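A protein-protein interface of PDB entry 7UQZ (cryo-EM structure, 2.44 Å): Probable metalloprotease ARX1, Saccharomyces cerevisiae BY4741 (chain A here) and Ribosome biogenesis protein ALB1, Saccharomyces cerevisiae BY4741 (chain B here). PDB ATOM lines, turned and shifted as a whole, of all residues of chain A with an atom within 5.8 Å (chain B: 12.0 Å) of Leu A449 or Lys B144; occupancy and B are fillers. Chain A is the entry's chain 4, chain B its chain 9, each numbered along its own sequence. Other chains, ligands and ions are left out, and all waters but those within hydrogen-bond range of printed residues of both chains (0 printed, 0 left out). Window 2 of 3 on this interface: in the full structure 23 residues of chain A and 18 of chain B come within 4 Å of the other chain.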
ATOM      1  N   PRO A 444      14.983  18.250  -1.497  1.00  0.00           N
ATOM      2  CA  PRO A 444      14.246  19.088  -0.544  1.00  0.00           C
ATOM      3  C   PRO A 444      13.315  20.071  -1.238  1.00  0.00           C
ATOM      4  O   PRO A 444      13.548  20.495  -2.372  1.00  0.00           O
ATOM      5  CB  PRO A 444      15.358  19.820   0.213  1.00  0.00           C
ATOM      6  CG  PRO A 444      16.495  19.848  -0.741  1.00  0.00           C
ATOM      7  CD  PRO A 444      16.422  18.557  -1.504  1.00  0.00           C
ATOM      8  N   TRP A 445      12.246  20.439  -0.525  1.00  0.00           N
ATOM      9  CA  TRP A 445      11.223  21.303  -1.107  1.00  0.00           C
ATOM     10  C   TRP A 445      11.694  22.743  -1.254  1.00  0.00           C
ATOM     11  O   TRP A 445      11.232  23.447  -2.157  1.00  0.00           O
ATOM     12  CB  TRP A 445       9.949  21.262  -0.267  1.00  0.00           C
ATOM     13  CG  TRP A 445       9.094  20.061  -0.511  1.00  0.00           C
ATOM     14  CD1 TRP A 445       8.881  19.023   0.343  1.00  0.00           C
ATOM     15  CD2 TRP A 445       8.332  19.775  -1.689  1.00  0.00           C
ATOM     16  NE1 TRP A 445       8.036  18.105  -0.227  1.00  0.00           N
ATOM     17  CE2 TRP A 445       7.685  18.543  -1.477  1.00  0.00           C
ATOM     18  CE3 TRP A 445       8.135  20.441  -2.903  1.00  0.00           C
ATOM     19  CZ2 TRP A 445       6.855  17.961  -2.432  1.00  0.00           C
ATOM     20  CZ3 TRP A 445       7.311  19.862  -3.849  1.00  0.00           C
ATOM     21  CH2 TRP A 445       6.681  18.635  -3.609  1.00  0.00           C
ATOM     22  N   ASP A 446      12.581  23.211  -0.371  1.00  0.00           N
ATOM     23  CA  ASP A 446      12.999  24.608  -0.429  1.00  0.00           C
ATOM     24  C   ASP A 446      13.809  24.896  -1.688  1.00  0.00           C
ATOM     25  O   ASP A 446      13.674  25.969  -2.284  1.00  0.00           O
ATOM     26  CB  ASP A 446      13.785  24.981   0.830  1.00  0.00           C
ATOM     27  CG  ASP A 446      14.923  24.026   1.118  1.00  0.00           C
ATOM     28  OD1 ASP A 446      15.053  23.016   0.399  1.00  0.00           O
ATOM     29  OD2 ASP A 446      15.689  24.291   2.066  1.00  0.00           O
ATOM     30  N   HIS A 447      14.643  23.945  -2.116  1.00  0.00           N
ATOM     31  CA  HIS A 447      15.379  24.107  -3.368  1.00  0.00           C
ATOM     32  C   HIS A 447      14.430  24.189  -4.560  1.00  0.00           C
ATOM     33  O   HIS A 447      14.620  25.017  -5.461  1.00  0.00           O
ATOM     34  CB  HIS A 447      16.366  22.952  -3.540  1.00  0.00           C
ATOM     35  CG  HIS A 447      17.186  23.034  -4.789  1.00  0.00           C
ATOM     36  ND1 HIS A 447      18.290  23.849  -4.903  1.00  0.00           N
ATOM     37  CD2 HIS A 447      17.061  22.401  -5.979  1.00  0.00           C
ATOM     38  CE1 HIS A 447      18.812  23.716  -6.109  1.00  0.00           C
ATOM     39  NE2 HIS A 447      18.086  22.842  -6.782  1.00  0.00           N
ATOM     40  N   ILE A 448      13.393  23.347  -4.571  1.00  0.00           N
ATOM     41  CA  ILE A 448      12.411  23.368  -5.652  1.00  0.00           C
ATOM     42  C   ILE A 448      11.656  24.691  -5.665  1.00  0.00           C
ATOM     43  O   ILE A 448      11.419  25.278  -6.728  1.00  0.00           O
ATOM     44  CB  ILE A 448      11.454  22.167  -5.521  1.00  0.00           C
ATOM     45  CG1 ILE A 448      12.225  20.851  -5.647  1.00  0.00           C
ATOM     46  CG2 ILE A 448      10.347  22.239  -6.561  1.00  0.00           C
ATOM     47  CD1 ILE A 448      11.356  19.618  -5.537  1.00  0.00           C
ATOM     48  N   LEU A 449      11.271  25.185  -4.486  1.00  0.00           N
ATOM     49  CA  LEU A 449      10.517  26.434  -4.418  1.00  0.00           C
ATOM     50  C   LEU A 449      11.381  27.632  -4.801  1.00  0.00           C
ATOM     51  O   LEU A 449      10.886  28.592  -5.402  1.00  0.00           O
ATOM     52  CB  LEU A 449       9.926  26.621  -3.022  1.00  0.00           C
ATOM     53  CG  LEU A 449       8.871  25.608  -2.569  1.00  0.00           C
ATOM     54  CD1 LEU A 449       8.405  25.929  -1.161  1.00  0.00           C
ATOM     55  CD2 LEU A 449       7.691  25.565  -3.529  1.00  0.00           C
ATOM     56  N   LYS A 450      12.671  27.602  -4.459  1.00  0.00           N
ATOM     57  CA  LYS A 450      13.560  28.693  -4.837  1.00  0.00           C
ATOM     58  C   LYS A 450      14.021  28.600  -6.284  1.00  0.00           C
ATOM     59  O   LYS A 450      14.548  29.583  -6.815  1.00  0.00           O
ATOM     60  CB  LYS A 450      14.779  28.732  -3.914  1.00  0.00           C
ATOM     61  CG  LYS A 450      14.457  29.098  -2.478  1.00  0.00           C
ATOM     62  CD  LYS A 450      15.700  29.048  -1.606  1.00  0.00           C
ATOM     63  CE  LYS A 450      15.352  29.237  -0.140  1.00  0.00           C
ATOM     64  NZ  LYS A 450      16.559  29.187   0.728  1.00  0.00           N
ATOM     65  N   ALA A 451      13.838  27.449  -6.926  1.00  0.00           N
ATOM     66  CA  ALA A 451      14.227  27.294  -8.317  1.00  0.00           C
ATOM     67  C   ALA A 451      13.333  28.122  -9.238  1.00  0.00           C
ATOM     68  O   ALA A 451      12.191  28.456  -8.913  1.00  0.00           O
ATOM     69  CB  ALA A 451      14.165  25.827  -8.725  1.00  0.00           C
ATOM     70  N   LEU A 478       2.898  23.121  -9.490  1.00  0.00           N
ATOM     71  CA  LEU A 478       4.023  24.041  -9.583  1.00  0.00           C
ATOM     72  C   LEU A 478       4.510  24.249 -11.009  1.00  0.00           C
ATOM     73  O   LEU A 478       5.349  25.128 -11.237  1.00  0.00           O
ATOM     74  CB  LEU A 478       5.187  23.544  -8.721  1.00  0.00           C
ATOM     75  CG  LEU A 478       5.020  23.699  -7.211  1.00  0.00           C
ATOM     76  CD1 LEU A 478       6.195  23.074  -6.485  1.00  0.00           C
ATOM     77  CD2 LEU A 478       4.878  25.165  -6.844  1.00  0.00           C
ATOM     78  N   SER B 138      -1.624  36.063  -7.736  1.00  0.00           N
ATOM     79  CA  SER B 138      -1.307  35.003  -8.686  1.00  0.00           C
ATOM     80  C   SER B 138      -1.482  33.627  -8.051  1.00  0.00           C
ATOM     81  O   SER B 138      -1.100  33.415  -6.899  1.00  0.00           O
ATOM     82  CB  SER B 138       0.120  35.164  -9.212  1.00  0.00           C
ATOM     83  OG  SER B 138       0.418  34.179 -10.187  1.00  0.00           O
ATOM     84  N   SER B 139      -2.067  32.699  -8.814  1.00  0.00           N
ATOM     85  CA  SER B 139      -2.313  31.355  -8.297  1.00  0.00           C
ATOM     86  C   SER B 139      -1.009  30.620  -8.013  1.00  0.00           C
ATOM     87  O   SER B 139      -0.909  29.884  -7.024  1.00  0.00           O
ATOM     88  CB  SER B 139      -3.177  30.564  -9.279  1.00  0.00           C
ATOM     89  OG  SER B 139      -3.504  29.289  -8.756  1.00  0.00           O
ATOM     90  N   LEU B 140      -0.001  30.801  -8.872  1.00  0.00           N
ATOM     91  CA  LEU B 140       1.309  30.212  -8.613  1.00  0.00           C
ATOM     92  C   LEU B 140       1.926  30.786  -7.344  1.00  0.00           C
ATOM     93  O   LEU B 140       2.536  30.053  -6.555  1.00  0.00           O
ATOM     94  CB  LEU B 140       2.236  30.437  -9.807  1.00  0.00           C
ATOM     95  CG  LEU B 140       3.679  29.962  -9.623  1.00  0.00           C
ATOM     96  CD1 LEU B 140       3.726  28.457  -9.421  1.00  0.00           C
ATOM     97  CD2 LEU B 140       4.546  30.379 -10.800  1.00  0.00           C
ATOM     98  N   THR B 141       1.774  32.096  -7.132  1.00  0.00           N
ATOM     99  CA  THR B 141       2.262  32.717  -5.906  1.00  0.00           C
ATOM    100  C   THR B 141       1.563  32.141  -4.682  1.00  0.00           C
ATOM    101  O   THR B 141       2.210  31.848  -3.670  1.00  0.00           O
ATOM    102  CB  THR B 141       2.065  34.234  -5.973  1.00  0.00           C
ATOM    103  OG1 THR B 141       2.831  34.771  -7.057  1.00  0.00           O
ATOM    104  CG2 THR B 141       2.505  34.897  -4.674  1.00  0.00           C
ATOM    105  N   LEU B 142       0.241  31.958  -4.761  1.00  0.00           N
ATOM    106  CA  LEU B 142      -0.500  31.387  -3.640  1.00  0.00           C
ATOM    107  C   LEU B 142      -0.062  29.955  -3.355  1.00  0.00           C
ATOM    108  O   LEU B 142       0.100  29.569  -2.191  1.00  0.00           O
ATOM    109  CB  LEU B 142      -2.002  31.442  -3.921  1.00  0.00           C
ATOM    110  CG  LEU B 142      -2.616  32.836  -4.061  1.00  0.00           C
ATOM    111  CD1 LEU B 142      -4.075  32.737  -4.472  1.00  0.00           C
ATOM    112  CD2 LEU B 142      -2.470  33.628  -2.767  1.00  0.00           C
ATOM    113  N   VAL B 143       0.138  29.155  -4.407  1.00  0.00           N
ATOM    114  CA  VAL B 143       0.575  27.772  -4.230  1.00  0.00           C
ATOM    115  C   VAL B 143       1.961  27.723  -3.595  1.00  0.00           C
ATOM    116  O   VAL B 143       2.209  26.939  -2.668  1.00  0.00           O
ATOM    117  CB  VAL B 143       0.540  27.022  -5.576  1.00  0.00           C
ATOM    118  CG1 VAL B 143       1.286  25.703  -5.481  1.00  0.00           C
ATOM    119  CG2 VAL B 143      -0.896  26.780  -6.008  1.00  0.00           C
ATOM    120  N   LYS B 144       2.884  28.563  -4.077  1.00  0.00           N
ATOM    121  CA  LYS B 144       4.231  28.581  -3.518  1.00  0.00           C
ATOM    122  C   LYS B 144       4.228  29.047  -2.068  1.00  0.00           C
ATOM    123  O   LYS B 144       4.958  28.497  -1.236  1.00  0.00           O
ATOM    124  CB  LYS B 144       5.147  29.460  -4.372  1.00  0.00           C
ATOM    125  CG  LYS B 144       5.459  28.870  -5.739  1.00  0.00           C
ATOM    126  CD  LYS B 144       6.306  29.810  -6.584  1.00  0.00           C
ATOM    127  CE  LYS B 144       7.751  29.828  -6.119  1.00  0.00           C
ATOM    128  NZ  LYS B 144       8.421  28.519  -6.343  1.00  0.00           N
ATOM    129  N   GLU B 145       3.409  30.052  -1.743  1.00  0.00           N
ATOM    130  CA  GLU B 145       3.302  30.502  -0.358  1.00  0.00           C
ATOM    131  C   GLU B 145       2.741  29.407   0.540  1.00  0.00           C
ATOM    132  O   GLU B 145       3.225  29.204   1.660  1.00  0.00           O
ATOM    133  CB  GLU B 145       2.434  31.758  -0.273  1.00  0.00           C
ATOM    134  CG  GLU B 145       3.109  33.025  -0.776  1.00  0.00           C
ATOM    135  CD  GLU B 145       4.165  33.551   0.178  1.00  0.00           C
ATOM    136  OE1 GLU B 145       4.174  33.131   1.355  1.00  0.00           O
ATOM    137  OE2 GLU B 145       4.987  34.387  -0.251  1.00  0.00           O
ATOM    138  N   ALA B 146       1.719  28.688   0.064  1.00  0.00           N
ATOM    139  CA  ALA B 146       1.147  27.601   0.851  1.00  0.00           C
ATOM    140  C   ALA B 146       2.164  26.492   1.087  1.00  0.00           C
ATOM    141  O   ALA B 146       2.282  25.976   2.205  1.00  0.00           O
ATOM    142  CB  ALA B 146      -0.097  27.049   0.159  1.00  0.00           C
ATOM    143  N   LEU B 147       2.917  26.117   0.048  1.00  0.00           N
ATOM    144  CA  LEU B 147       3.926  25.073   0.204  1.00  0.00           C
ATOM    145  C   LEU B 147       5.040  25.515   1.146  1.00  0.00           C
ATOM    146  O   LEU B 147       5.516  24.725   1.970  1.00  0.00           O
ATOM    147  CB  LEU B 147       4.494  24.682  -1.160  1.00  0.00           C
ATOM    148  CG  LEU B 147       3.556  23.909  -2.089  1.00  0.00           C
ATOM    149  CD1 LEU B 147       4.172  23.767  -3.465  1.00  0.00           C
ATOM    150  CD2 LEU B 147       3.234  22.544  -1.508  1.00  0.00           C
ATOM    151  N   TRP B 148       5.465  26.778   1.038  1.00  0.00           N
ATOM    152  CA  TRP B 148       6.491  27.305   1.930  1.00  0.00           C
ATOM    153  C   TRP B 148       6.022  27.299   3.379  1.00  0.00           C
ATOM    154  O   TRP B 148       6.780  26.932   4.284  1.00  0.00           O
ATOM    155  CB  TRP B 148       6.872  28.720   1.493  1.00  0.00           C
ATOM    156  CG  TRP B 148       7.958  29.354   2.306  1.00  0.00           C
ATOM    157  CD1 TRP B 148       7.804  30.113   3.429  1.00  0.00           C
ATOM    158  CD2 TRP B 148       9.366  29.300   2.046  1.00  0.00           C
ATOM    159  NE1 TRP B 148       9.030  30.529   3.890  1.00  0.00           N
ATOM    160  CE2 TRP B 148      10.005  30.043   3.059  1.00  0.00           C
ATOM    161  CE3 TRP B 148      10.149  28.690   1.060  1.00  0.00           C
ATOM    162  CZ2 TRP B 148      11.390  30.195   3.114  1.00  0.00           C
ATOM    163  CZ3 TRP B 148      11.522  28.841   1.114  1.00  0.00           C
ATOM    164  CH2 TRP B 148      12.129  29.588   2.135  1.00  0.00           C
ATOM    165  N   SER B 149       4.769  27.692   3.615  1.00  0.00           N
ATOM    166  CA  SER B 149       4.250  27.718   4.976  1.00  0.00           C
ATOM    167  C   SER B 149       4.049  26.315   5.534  1.00  0.00           C
ATOM    168  O   SER B 149       4.216  26.101   6.740  1.00  0.00           O
ATOM    169  CB  SER B 149       2.943  28.505   5.021  1.00  0.00           C
ATOM    170  OG  SER B 149       3.147  29.842   4.599  1.00  0.00           O
ATOM    171  N   VAL B 150       3.682  25.353   4.684  1.00  0.00           N
ATOM    172  CA  VAL B 150       3.558  23.975   5.150  1.00  0.00           C
ATOM    173  C   VAL B 150       4.914  23.356   5.469  1.00  0.00           C
ATOM    174  O   VAL B 150       5.051  22.688   6.503  1.00  0.00           O
ATOM    175  CB  VAL B 150       2.797  23.125   4.117  1.00  0.00           C
ATOM    176  CG1 VAL B 150       2.890  21.649   4.455  1.00  0.00           C
ATOM    177  CG2 VAL B 150       1.342  23.545   4.069  1.00  0.00           C
ATOM    178  N   ILE B 151       5.934  23.582   4.638  1.00  0.00           N
ATOM    179  CA  ILE B 151       7.244  22.998   4.917  1.00  0.00           C
ATOM    180  C   ILE B 151       8.009  23.751   6.001  1.00  0.00           C
ATOM    181  O   ILE B 151       8.942  23.185   6.589  1.00  0.00           O
ATOM    182  CB  ILE B 151       8.117  22.915   3.651  1.00  0.00           C
ATOM    183  CG1 ILE B 151       8.500  24.312   3.159  1.00  0.00           C
ATOM    184  CG2 ILE B 151       7.411  22.115   2.563  1.00  0.00           C
ATOM    185  CD1 ILE B 151       9.460  24.302   1.995  1.00  0.00           C
ATOM    186  N   ASP B 152       7.645  24.997   6.291  1.00  0.00           N
ATOM    187  CA  ASP B 152       8.293  25.736   7.369  1.00  0.00           C
ATOM    188  C   ASP B 152       7.766  25.285   8.727  1.00  0.00           C
ATOM    189  O   ASP B 152       8.119  24.215   9.220  1.00  0.00           O
ATOM    190  CB  ASP B 152       8.083  27.241   7.199  1.00  0.00           C
ATOM    191  CG  ASP B 152       8.836  28.056   8.235  1.00  0.00           C
ATOM    192  OD1 ASP B 152       9.860  27.564   8.755  1.00  0.00           O
ATOM    193  OD2 ASP B 152       8.401  29.188   8.533  1.00  0.00           O
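Hydrophobic or aromatic side chains of chain A within 4 Å of the printed part of chain B: Trp A445, Leu A449 and Leu A478. Hydrophobic or aromatic side chains of chain B that line the printed part of chain A: Val B143, Leu B147, Trp B148 and Ile B151. Among the printed residues, 9 pairs touch across the chains. Among the printed residues, no Asp or Glu carboxylate lies within 4 Å of a Lys or Arg side-chain nitrogen of the other chain.
Leu A449 touches four residues of chain B. Printed residues of chain B within 4 Å of Trp A445: Ile B151. No residue of chain B comes within 4 Å of Ile A448. Of chain B, only Trp B148 comes within 4 Å of Lys A450. Ala A451 touches none of the printed residues of chain B. Leu A478 touches just these residues of chain B: Val B143, Lys B144 and Leu B147. Printed residues of chain A within 4 Å of Ile B151: Trp A445 (3.8 Å) and Leu A449 (3.7 Å). Printed residues of chain A within 4 Å of Val B143: Leu A478. Printed residues of chain A within 4 Å of Leu B147: Leu A449 (3.95 Å) and Leu A478 (3.7 Å). The nearest residue of chain B that does not touch Leu A449 is Val B143 (5.7 Å). The nearest residue of chain A that does not touch Lys B144 is Ile A448 (4.4 Å).
O of Leu A449 lies within hydrogen-bond range of NZ of Lys B144, 2.6 Å away.
CD1 of Ile B151 touches CB of Trp A445 (3.8 Å). Leu A449 touches Leu B147. N of Trp B148 touches CD1 of Leu A449, 3.8 Å away. Leu A449 touches Ile B151. Lys A450 touches Trp B148 (CE to CH2, 3.96 Å). Leu A478 touches Val B143 (CD2 to CG1, 3.9 Å). Lys B144 touches Leu A478 (CG to CD2, 3.9 Å). Leu B147 touches Leu A478.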
